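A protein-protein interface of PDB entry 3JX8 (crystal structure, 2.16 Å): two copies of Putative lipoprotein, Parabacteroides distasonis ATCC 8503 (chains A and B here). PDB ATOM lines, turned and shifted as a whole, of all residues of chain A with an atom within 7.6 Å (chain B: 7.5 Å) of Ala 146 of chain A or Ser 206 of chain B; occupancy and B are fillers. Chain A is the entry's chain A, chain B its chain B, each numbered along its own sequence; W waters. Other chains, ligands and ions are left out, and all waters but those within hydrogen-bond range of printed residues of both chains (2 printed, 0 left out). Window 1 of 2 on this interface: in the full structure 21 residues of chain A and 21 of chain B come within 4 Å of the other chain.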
ATOM      1  N   THR A 103      25.117  14.759  25.781  1.00  0.00           N
ATOM      2  CA  THR A 103      24.179  14.834  26.858  1.00  0.00           C
ATOM      3  C   THR A 103      23.440  13.480  27.032  1.00  0.00           C
ATOM      4  O   THR A 103      23.077  12.818  26.035  1.00  0.00           O
ATOM      5  CB  THR A 103      23.210  16.004  26.630  1.00  0.00           C
ATOM      6  OG1 THR A 103      22.409  16.159  27.794  1.00  0.00           O
ATOM      7  CG2 THR A 103      22.316  15.798  25.449  1.00  0.00           C
ATOM      8  N   VAL A 104      23.269  13.060  28.284  1.00  0.00           N
ATOM      9  CA  VAL A 104      22.683  11.772  28.615  1.00  0.00           C
ATOM     10  C   VAL A 104      21.766  11.958  29.804  1.00  0.00           C
ATOM     11  O   VAL A 104      22.187  12.468  30.860  1.00  0.00           O
ATOM     12  CB  VAL A 104      23.759  10.694  28.986  1.00  0.00           C
ATOM     13  CG1 VAL A 104      23.080   9.342  29.311  1.00  0.00           C
ATOM     14  CG2 VAL A 104      24.838  10.531  27.860  1.00  0.00           C
ATOM     15  N   ASN A 123      24.903  15.307  20.514  1.00  0.00           N
ATOM     16  CA  ASN A 123      24.698  13.873  20.754  1.00  0.00           C
ATOM     17  C   ASN A 123      23.924  13.705  22.064  1.00  0.00           C
ATOM     18  O   ASN A 123      24.398  14.101  23.131  1.00  0.00           O
ATOM     19  CB  ASN A 123      26.019  13.130  20.852  1.00  0.00           C
ATOM     20  CG  ASN A 123      26.878  13.265  19.597  1.00  0.00           C
ATOM     21  OD1 ASN A 123      26.453  12.930  18.493  1.00  0.00           O
ATOM     22  ND2 ASN A 123      28.107  13.718  19.779  1.00  0.00           N
ATOM     23  N   MET A 124      22.715  13.179  21.967  1.00  0.00           N
ATOM     24  CA  MET A 124      21.875  12.886  23.118  1.00  0.00           C
ATOM     25  C   MET A 124      21.507  11.391  23.269  1.00  0.00           C
ATOM     26  O   MET A 124      21.103  10.753  22.297  1.00  0.00           O
ATOM     27  CB  MET A 124      20.603  13.660  22.998  1.00  0.00           C
ATOM     28  CG  MET A 124      19.398  12.930  23.698  1.00  0.00           C
ATOM     29  SD  MET A 124      18.487  14.354  24.483  1.00  0.00           S
ATOM     30  CE  MET A 124      19.135  14.107  26.370  1.00  0.00           C
ATOM     31  N   ALA A 125      21.633  10.851  24.487  1.00  0.00           N
ATOM     32  CA  ALA A 125      21.090   9.547  24.819  1.00  0.00           C
ATOM     33  C   ALA A 125      20.093   9.733  25.964  1.00  0.00           C
ATOM     34  O   ALA A 125      20.400  10.372  26.975  1.00  0.00           O
ATOM     35  CB  ALA A 125      22.208   8.566  25.189  1.00  0.00           C
ATOM     36  N   GLY A 126      18.889   9.209  25.794  1.00  0.00           N
ATOM     37  CA  GLY A 126      17.882   9.203  26.829  1.00  0.00           C
ATOM     38  C   GLY A 126      16.547   9.845  26.487  1.00  0.00           C
ATOM     39  O   GLY A 126      16.176  10.010  25.312  1.00  0.00           O
ATOM     40  N   SER A 127      15.821  10.199  27.549  1.00  0.00           N
ATOM     41  CA  SER A 127      14.454  10.655  27.485  1.00  0.00           C
ATOM     42  C   SER A 127      14.356  12.150  27.525  1.00  0.00           C
ATOM     43  O   SER A 127      13.268  12.700  27.400  1.00  0.00           O
ATOM     44  CB  SER A 127      13.687  10.097  28.666  1.00  0.00           C
ATOM     45  OG  SER A 127      14.306  10.534  29.895  1.00  0.00           O
ATOM     46  N   ASN A 144      22.325  14.096  16.701  1.00  0.00           N
ATOM     47  CA  ASN A 144      22.273  12.679  16.846  1.00  0.00           C
ATOM     48  C   ASN A 144      21.602  12.339  18.131  1.00  0.00           C
ATOM     49  O   ASN A 144      21.919  12.922  19.195  1.00  0.00           O
ATOM     50  CB  ASN A 144      23.671  12.139  16.846  1.00  0.00           C
ATOM     51  CG  ASN A 144      24.422  12.542  15.609  1.00  0.00           C
ATOM     52  OD1 ASN A 144      23.866  12.508  14.505  1.00  0.00           O
ATOM     53  ND2 ASN A 144      25.670  12.957  15.777  1.00  0.00           N
ATOM     54  N   MET A 145      20.671  11.405  18.061  1.00  0.00           N
ATOM     55  CA  MET A 145      20.094  10.886  19.283  1.00  0.00           C
ATOM     56  C   MET A 145      19.761   9.387  19.305  1.00  0.00           C
ATOM     57  O   MET A 145      19.468   8.751  18.247  1.00  0.00           O
ATOM     58  CB  MET A 145      18.905  11.710  19.678  1.00  0.00           C
ATOM     59  CG  MET A 145      17.712  11.583  18.823  1.00  0.00           C
ATOM     60  SD  MET A 145      16.204  12.015  20.027  1.00  0.00           S
ATOM     61  CE  MET A 145      16.233  10.429  21.170  1.00  0.00           C
ATOM     62  N   ALA A 146      19.882   8.815  20.508  1.00  0.00           N
ATOM     63  CA  ALA A 146      19.497   7.439  20.753  1.00  0.00           C
ATOM     64  C   ALA A 146      18.636   7.462  21.999  1.00  0.00           C
ATOM     65  O   ALA A 146      19.113   7.742  23.127  1.00  0.00           O
ATOM     66  CB  ALA A 146      20.727   6.522  20.919  1.00  0.00           C
ATOM     67  N   GLY A 147      17.354   7.207  21.807  1.00  0.00           N
ATOM     68  CA  GLY A 147      16.441   7.128  22.926  1.00  0.00           C
ATOM     69  C   GLY A 147      15.068   7.601  22.564  1.00  0.00           C
ATOM     70  O   GLY A 147      14.736   7.707  21.389  1.00  0.00           O
ATOM     71  N   SER A 148      14.282   7.866  23.606  1.00  0.00           N
ATOM     72  CA  SER A 148      12.897   8.261  23.472  1.00  0.00           C
ATOM     73  C   SER A 148      12.677   9.768  23.604  1.00  0.00           C
ATOM     74  O   SER A 148      11.561  10.252  23.476  1.00  0.00           O
ATOM     75  CB  SER A 148      12.074   7.543  24.539  1.00  0.00           C
ATOM     76  OG  SER A 148      12.473   7.986  25.822  1.00  0.00           O
ATOM     77  N   GLY A 149      13.730  10.512  23.881  1.00  0.00           N
ATOM     78  CA  GLY A 149      13.580  11.950  24.019  1.00  0.00           C
ATOM     79  C   GLY A 149      13.522  12.687  22.690  1.00  0.00           C
ATOM     80  O   GLY A 149      13.168  12.118  21.646  1.00  0.00           O
ATOM     81  N   ILE A 151      15.111  16.281  20.174  1.00  0.00           N
ATOM     82  CA  ILE A 151      15.919  17.448  19.829  1.00  0.00           C
ATOM     83  C   ILE A 151      15.058  18.290  18.913  1.00  0.00           C
ATOM     84  O   ILE A 151      14.416  17.740  18.011  1.00  0.00           O
ATOM     85  CB  ILE A 151      17.177  17.058  19.057  1.00  0.00           C
ATOM     86  CG1 ILE A 151      18.049  16.090  19.892  1.00  0.00           C
ATOM     87  CG2 ILE A 151      17.950  18.300  18.643  1.00  0.00           C
ATOM     88  CD1 ILE A 151      19.336  15.596  19.184  1.00  0.00           C
ATOM     89  N   SER A 164      20.505  11.997  12.806  1.00  0.00           N
ATOM     90  CA  SER A 164      20.385  10.560  12.967  1.00  0.00           C
ATOM     91  C   SER A 164      19.693  10.256  14.284  1.00  0.00           C
ATOM     92  O   SER A 164      20.118  10.712  15.358  1.00  0.00           O
ATOM     93  CB  SER A 164      21.742   9.919  12.969  1.00  0.00           C
ATOM     94  OG  SER A 164      22.435  10.304  11.813  1.00  0.00           O
ATOM     95  N   LEU A 165      18.650   9.451  14.189  1.00  0.00           N
ATOM     96  CA  LEU A 165      17.792   9.089  15.298  1.00  0.00           C
ATOM     97  C   LEU A 165      17.793   7.571  15.423  1.00  0.00           C
ATOM     98  O   LEU A 165      17.461   6.867  14.459  1.00  0.00           O
ATOM     99  CB  LEU A 165      16.377   9.591  14.990  1.00  0.00           C
ATOM    100  CG  LEU A 165      15.199   9.156  15.853  1.00  0.00           C
ATOM    101  CD1 LEU A 165      15.499   9.270  17.324  1.00  0.00           C
ATOM    102  CD2 LEU A 165      13.992  10.027  15.450  1.00  0.00           C
ATOM    103  N   ALA A 166      18.232   7.051  16.569  1.00  0.00           N
ATOM    104  CA  ALA A 166      18.076   5.623  16.889  1.00  0.00           C
ATOM    105  C   ALA A 166      16.974   5.550  17.922  1.00  0.00           C
ATOM    106  O   ALA A 166      16.890   6.394  18.829  1.00  0.00           O
ATOM    107  CB  ALA A 166      19.387   4.987  17.424  1.00  0.00           C
ATOM    108  N   SER A 167      16.131   4.535  17.791  1.00  0.00           N
ATOM    109  CA  SER A 167      15.054   4.263  18.734  1.00  0.00           C
ATOM    110  C   SER A 167      13.812   5.103  18.463  1.00  0.00           C
ATOM    111  O   SER A 167      13.521   5.412  17.309  1.00  0.00           O
ATOM    112  CB  SER A 167      15.526   4.346  20.200  1.00  0.00           C
ATOM    113  OG  SER A 167      14.707   3.533  21.042  1.00  0.00           O
ATOM    114  N   SER A 168      13.067   5.441  19.509  1.00  0.00           N
ATOM    115  CA  SER A 168      11.671   5.857  19.366  1.00  0.00           C
ATOM    116  C   SER A 168      11.409   7.349  19.476  1.00  0.00           C
ATOM    117  O   SER A 168      10.263   7.776  19.376  1.00  0.00           O
ATOM    118  CB  SER A 168      10.828   5.136  20.441  1.00  0.00           C
ATOM    119  OG  SER A 168      11.274   5.508  21.731  1.00  0.00           O
ATOM    120  N   GLY A 169      12.453   8.137  19.683  1.00  0.00           N
ATOM    121  CA  GLY A 169      12.302   9.568  19.893  1.00  0.00           C
ATOM    122  C   GLY A 169      11.949  10.405  18.660  1.00  0.00           C
ATOM    123  O   GLY A 169      11.405   9.907  17.651  1.00  0.00           O
ATOM    124  N   ILE A 171      13.233  14.109  16.335  1.00  0.00           N
ATOM    125  CA  ILE A 171      14.036  15.251  15.983  1.00  0.00           C
ATOM    126  C   ILE A 171      13.165  16.116  15.107  1.00  0.00           C
ATOM    127  O   ILE A 171      12.533  15.600  14.166  1.00  0.00           O
ATOM    128  CB  ILE A 171      15.312  14.885  15.230  1.00  0.00           C
ATOM    129  CG1 ILE A 171      16.151  13.919  16.064  1.00  0.00           C
ATOM    130  CG2 ILE A 171      16.113  16.165  14.869  1.00  0.00           C
ATOM    131  CD1 ILE A 171      17.418  13.431  15.390  1.00  0.00           C
ATOM    132  N   SER B 167      16.925  -0.632  17.772  1.00  0.00           N
ATOM    133  CA  SER B 167      15.565  -0.771  18.270  1.00  0.00           C
ATOM    134  C   SER B 167      15.445  -1.829  19.364  1.00  0.00           C
ATOM    135  O   SER B 167      16.381  -2.036  20.132  1.00  0.00           O
ATOM    136  CB  SER B 167      14.536  -0.929  17.145  1.00  0.00           C
ATOM    137  OG  SER B 167      13.271  -0.474  17.596  1.00  0.00           O
ATOM    138  N   VAL B 184      24.329  -2.328  20.621  1.00  0.00           N
ATOM    139  CA  VAL B 184      22.904  -2.080  20.772  1.00  0.00           C
ATOM    140  C   VAL B 184      22.661  -0.579  20.746  1.00  0.00           C
ATOM    141  O   VAL B 184      23.326   0.152  21.466  1.00  0.00           O
ATOM    142  CB  VAL B 184      22.382  -2.618  22.079  1.00  0.00           C
ATOM    143  CG1 VAL B 184      20.922  -2.244  22.230  1.00  0.00           C
ATOM    144  CG2 VAL B 184      22.628  -4.143  22.164  1.00  0.00           C
ATOM    145  N   ALA B 185      21.740  -0.125  19.902  1.00  0.00           N
ATOM    146  CA  ALA B 185      21.330   1.283  19.880  1.00  0.00           C
ATOM    147  C   ALA B 185      19.830   1.262  20.042  1.00  0.00           C
ATOM    148  O   ALA B 185      19.081   1.172  19.078  1.00  0.00           O
ATOM    149  CB  ALA B 185      21.759   2.006  18.575  1.00  0.00           C
ATOM    150  N   GLY B 186      19.378   1.341  21.274  1.00  0.00           N
ATOM    151  CA  GLY B 186      17.964   1.140  21.546  1.00  0.00           C
ATOM    152  C   GLY B 186      17.774   0.383  22.821  1.00  0.00           C
ATOM    153  O   GLY B 186      18.691   0.305  23.651  1.00  0.00           O
ATOM    154  N   SER B 187      16.588  -0.173  22.962  1.00  0.00           N
ATOM    155  CA  SER B 187      16.155  -0.803  24.181  1.00  0.00           C
ATOM    156  C   SER B 187      16.326  -2.309  24.095  1.00  0.00           C
ATOM    157  O   SER B 187      16.038  -3.015  25.049  1.00  0.00           O
ATOM    158  CB  SER B 187      14.655  -0.472  24.429  1.00  0.00           C
ATOM    159  OG  SER B 187      13.854  -1.019  23.360  1.00  0.00           O
ATOM    160  N   GLY B 188      16.777  -2.813  22.971  1.00  0.00           N
ATOM    161  CA  GLY B 188      16.923  -4.246  22.795  1.00  0.00           C
ATOM    162  C   GLY B 188      18.072  -4.912  23.553  1.00  0.00           C
ATOM    163  O   GLY B 188      18.786  -4.293  24.371  1.00  0.00           O
ATOM    164  N   ILE B 204      26.755   0.028  24.070  1.00  0.00           N
ATOM    165  CA  ILE B 204      25.340   0.364  24.203  1.00  0.00           C
ATOM    166  C   ILE B 204      25.111   1.860  24.114  1.00  0.00           C
ATOM    167  O   ILE B 204      25.772   2.654  24.817  1.00  0.00           O
ATOM    168  CB  ILE B 204      24.736  -0.155  25.510  1.00  0.00           C
ATOM    169  CG1 ILE B 204      24.977  -1.682  25.629  1.00  0.00           C
ATOM    170  CG2 ILE B 204      23.196   0.153  25.577  1.00  0.00           C
ATOM    171  CD1 ILE B 204      24.594  -2.311  26.960  1.00  0.00           C
ATOM    172  N   ALA B 205      24.168   2.225  23.250  1.00  0.00           N
ATOM    173  CA  ALA B 205      23.585   3.555  23.215  1.00  0.00           C
ATOM    174  C   ALA B 205      22.117   3.450  23.701  1.00  0.00           C
ATOM    175  O   ALA B 205      21.326   2.677  23.168  1.00  0.00           O
ATOM    176  CB  ALA B 205      23.663   4.176  21.783  1.00  0.00           C
ATOM    177  N   SER B 206      21.776   4.281  24.681  1.00  0.00           N
ATOM    178  CA  SER B 206      20.501   4.295  25.414  1.00  0.00           C
ATOM    179  C   SER B 206      20.314   3.094  26.347  1.00  0.00           C
ATOM    180  O   SER B 206      21.235   2.804  27.121  1.00  0.00           O
ATOM    181  CB  SER B 206      19.291   4.610  24.527  1.00  0.00           C
ATOM    182  OG  SER B 206      18.802   3.488  23.865  1.00  0.00           O
ATOM    183  N   SER B 207      19.166   2.419  26.331  1.00  0.00           N
ATOM    184  CA  SER B 207      18.766   1.560  27.483  1.00  0.00           C
ATOM    185  C   SER B 207      18.894   0.046  27.302  1.00  0.00           C
ATOM    186  O   SER B 207      18.503  -0.740  28.195  1.00  0.00           O
ATOM    187  CB  SER B 207      17.319   1.873  27.852  1.00  0.00           C
ATOM    188  OG  SER B 207      16.459   1.539  26.779  1.00  0.00           O
ATOM    189  N   GLY B 208      19.472  -0.385  26.191  1.00  0.00           N
ATOM    190  CA  GLY B 208      19.633  -1.811  25.946  1.00  0.00           C
ATOM    191  C   GLY B 208      20.612  -2.554  26.867  1.00  0.00           C
ATOM    192  O   GLY B 208      21.201  -1.991  27.804  1.00  0.00           O
ATOM    193  N   GLU B 209      20.744  -3.844  26.594  1.00  0.00           N
ATOM    194  CA  GLU B 209      21.544  -4.745  27.390  1.00  0.00           C
ATOM    195  C   GLU B 209      22.340  -5.693  26.535  1.00  0.00           C
ATOM    196  O   GLU B 209      21.860  -6.159  25.494  1.00  0.00           O
ATOM    197  CB  GLU B 209      20.672  -5.668  28.219  1.00  0.00           C
ATOM    198  CG  GLU B 209      20.015  -5.118  29.411  1.00  0.00           C
ATOM    199  CD  GLU B 209      19.408  -6.279  30.204  1.00  0.00           C
ATOM    200  OE1 GLU B 209      18.478  -6.926  29.670  1.00  0.00           O
ATOM    201  OE2 GLU B 209      19.907  -6.592  31.295  1.00  0.00           O
ATOM    202  N   ILE B 222      29.174   2.109  27.545  1.00  0.00           N
ATOM    203  CA  ILE B 222      27.752   2.439  27.647  1.00  0.00           C
ATOM    204  C   ILE B 222      27.651   3.953  27.565  1.00  0.00           C
ATOM    205  O   ILE B 222      28.406   4.656  28.250  1.00  0.00           O
ATOM    206  CB  ILE B 222      27.111   1.949  28.948  1.00  0.00           C
ATOM    207  CG1 ILE B 222      27.358   0.439  29.131  1.00  0.00           C
ATOM    208  CG2 ILE B 222      25.636   2.286  28.964  1.00  0.00           C
ATOM    209  CD1 ILE B 222      26.902  -0.151  30.482  1.00  0.00           C
ATOM    210  N   VAL B 223      26.761   4.422  26.680  1.00  0.00           N
ATOM    211  CA  VAL B 223      26.259   5.789  26.698  1.00  0.00           C
ATOM    212  C   VAL B 223      24.724   5.723  26.908  1.00  0.00           C
ATOM    213  O   VAL B 223      23.994   5.409  26.004  1.00  0.00           O
ATOM    214  CB  VAL B 223      26.632   6.562  25.387  1.00  0.00           C
ATOM    215  CG1 VAL B 223      26.194   8.035  25.507  1.00  0.00           C
ATOM    216  CG2 VAL B 223      28.174   6.439  25.067  1.00  0.00           C
ATOM    217  N   GLY B 224      24.251   5.977  28.121  1.00  0.00           N
ATOM    218  CA  GLY B 224      22.837   5.865  28.461  1.00  0.00           C
ATOM    219  C   GLY B 224      22.631   5.107  29.761  1.00  0.00           C
ATOM    220  O   GLY B 224      23.488   5.078  30.621  1.00  0.00           O
ATOM    221  N   SER B 225      21.474   4.489  29.896  1.00  0.00           N
ATOM    222  CA  SER B 225      21.071   3.781  31.091  1.00  0.00           C
ATOM    223  C   SER B 225      21.210   2.259  30.944  1.00  0.00           C
ATOM    224  O   SER B 225      20.858   1.520  31.841  1.00  0.00           O
ATOM    225  CB  SER B 225      19.598   4.118  31.344  1.00  0.00           C
ATOM    226  OG  SER B 225      18.826   3.666  30.242  1.00  0.00           O
ATOM    227  N   GLY B 226      21.711   1.798  29.806  1.00  0.00           N
ATOM    228  CA  GLY B 226      21.873   0.383  29.538  1.00  0.00           C
ATOM    229  C   GLY B 226      22.886  -0.320  30.442  1.00  0.00           C
ATOM    230  O   GLY B 226      23.536   0.285  31.309  1.00  0.00           O
ATOM    231  N   GLU B 227      22.974  -1.626  30.253  1.00  0.00           N
ATOM    232  CA  GLU B 227      23.722  -2.507  31.143  1.00  0.00           C
ATOM    233  C   GLU B 227      24.478  -3.561  30.395  1.00  0.00           C
ATOM    234  O   GLU B 227      23.939  -4.159  29.455  1.00  0.00           O
ATOM    235  CB  GLU B 227      22.757  -3.195  32.114  1.00  0.00           C
ATOM    236  CG  GLU B 227      22.024  -2.214  32.972  1.00  0.00           C
ATOM    237  CD  GLU B 227      21.097  -2.862  34.010  1.00  0.00           C
ATOM    238  OE1 GLU B 227      21.350  -3.967  34.506  1.00  0.00           O
ATOM    239  OE2 GLU B 227      20.108  -2.218  34.362  1.00  0.00           O
ATOM    240  N   MET B 241      28.968   6.569  30.324  1.00  0.00           N
ATOM    241  CA  MET B 241      28.475   7.928  30.363  1.00  0.00           C
ATOM    242  C   MET B 241      26.951   7.845  30.501  1.00  0.00           C
ATOM    243  O   MET B 241      26.259   7.541  29.547  1.00  0.00           O
ATOM    244  CB  MET B 241      28.858   8.696  29.101  1.00  0.00           C
ATOM    245  CG  MET B 241      28.485  10.145  29.205  1.00  0.00           C
ATOM    246  SD  MET B 241      28.606  11.092  27.495  1.00  0.00           S
ATOM    247  CE  MET B 241      30.569  10.941  27.287  1.00  0.00           C
ATOM    248  N   SER B 243      23.594   6.706  33.538  1.00  0.00           N
ATOM    249  CA  SER B 243      23.173   5.947  34.708  1.00  0.00           C
ATOM    250  C   SER B 243      23.339   4.431  34.522  1.00  0.00           C
ATOM    251  O   SER B 243      22.963   3.651  35.395  1.00  0.00           O
ATOM    252  CB  SER B 243      21.665   6.218  34.931  1.00  0.00           C
ATOM    253  OG  SER B 243      20.969   5.859  33.714  1.00  0.00           O
ATOM    254  N   GLY B 244      23.854   4.006  33.380  1.00  0.00           N
ATOM    255  CA  GLY B 244      24.050   2.593  33.096  1.00  0.00           C
ATOM    256  C   GLY B 244      25.053   1.911  34.021  1.00  0.00           C
ATOM    257  O   GLY B 244      25.695   2.528  34.874  1.00  0.00           O
HETATM  258  O   HOH W   1      14.437   0.813  21.034  1.00  0.00           O
HETATM  259  O   HOH W   2      15.858   3.589  23.714  1.00  0.00           O
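Hydrophobic or aromatic side chains of chain A within 4 Å of the printed part of chain B: Val 104, Ala 125, Ala 146 and Ala 166. Hydrophobic or aromatic side chains of chain B that line the printed part of chain A: Ala 185, Ala 205, Val 223 and Met 241. Among the printed residues, no Asp or Glu carboxylate lies within 4 Å of a Lys or Arg side-chain nitrogen of the other chain.
Position printed for both chains: 167.
N of Ser 206 of chain B sits at hydrogen-bond distance from O of Val 223 of chain B (2.8 Å). O of Ser 206 of chain B is in hydrogen-bond range of N of Ser 225 of chain B (3.3 Å). The backbone carbonyl oxygen (O) of Thr 103 of chain A sits at hydrogen-bond distance from the backbone NH (N) of Ala 125 of chain A, at 2.9 Å. N of Ala 166 of chain A is in hydrogen-bond range of O of Met 145 of chain A, at 2.7 Å. N of Gly 186 of chain B sits at hydrogen-bond distance from O of Ala 205 of chain B. O of Ala 166 of chain A lies within hydrogen-bond range of N of Gly 147 of chain A, at 3.1 Å.
Water W1 bridges the side-chain hydroxyl of Ser 167 of chain A (2.7 Å) and the side-chain hydroxyl of Ser 187 of chain B (3.0 Å). Water W2 lies within hydrogen-bond range of the side-chain hydroxyl of Ser 167 of chain A (2.9 Å) and the side-chain hydroxyl of Ser 206 of chain B (2.9 Å).
Ser 206 of chain B touches one residue of chain A. Ala 205 of chain B touches just one residue of chain A: Ala 146 (3.9 Å). Of the printed residues of chain B, Ala 166 of chain A touches Ala 185 (3.98 Å). Of the printed residues of chain A, Gly 224 of chain B touches Val 104. Printed residues of chain A within 4 Å of Met 241 of chain B: Val 104 (3.7 Å). The nearest residue of chain B that does not touch Ala 146 of chain A is Ala 185 of chain B (5.2 Å). The nearest residue of chain A that does not touch Ser 206 of chain B is Gly 147 of chain A (4.1 Å).
Val 104 of chain A touches Val 223 of chain B. Gly 224 of chain B touches Val 104 of chain A (CA to CG1, 3.6 Å). Val 104 of chain A touches Met 241 of chain B (CG1 to O, 3.7 Å). O of Val 223 of chain B touches CB of Ala 125 of chain A (3.7 Å). CB of Ala 205 of chain B touches CB of Ala 146 of chain A, at 3.9 Å. Ala 146 of chain A touches Ser 206 of chain B. Ala 166 of chain A touches Ala 185 of chain B (CB to CB, 3.98 Å).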
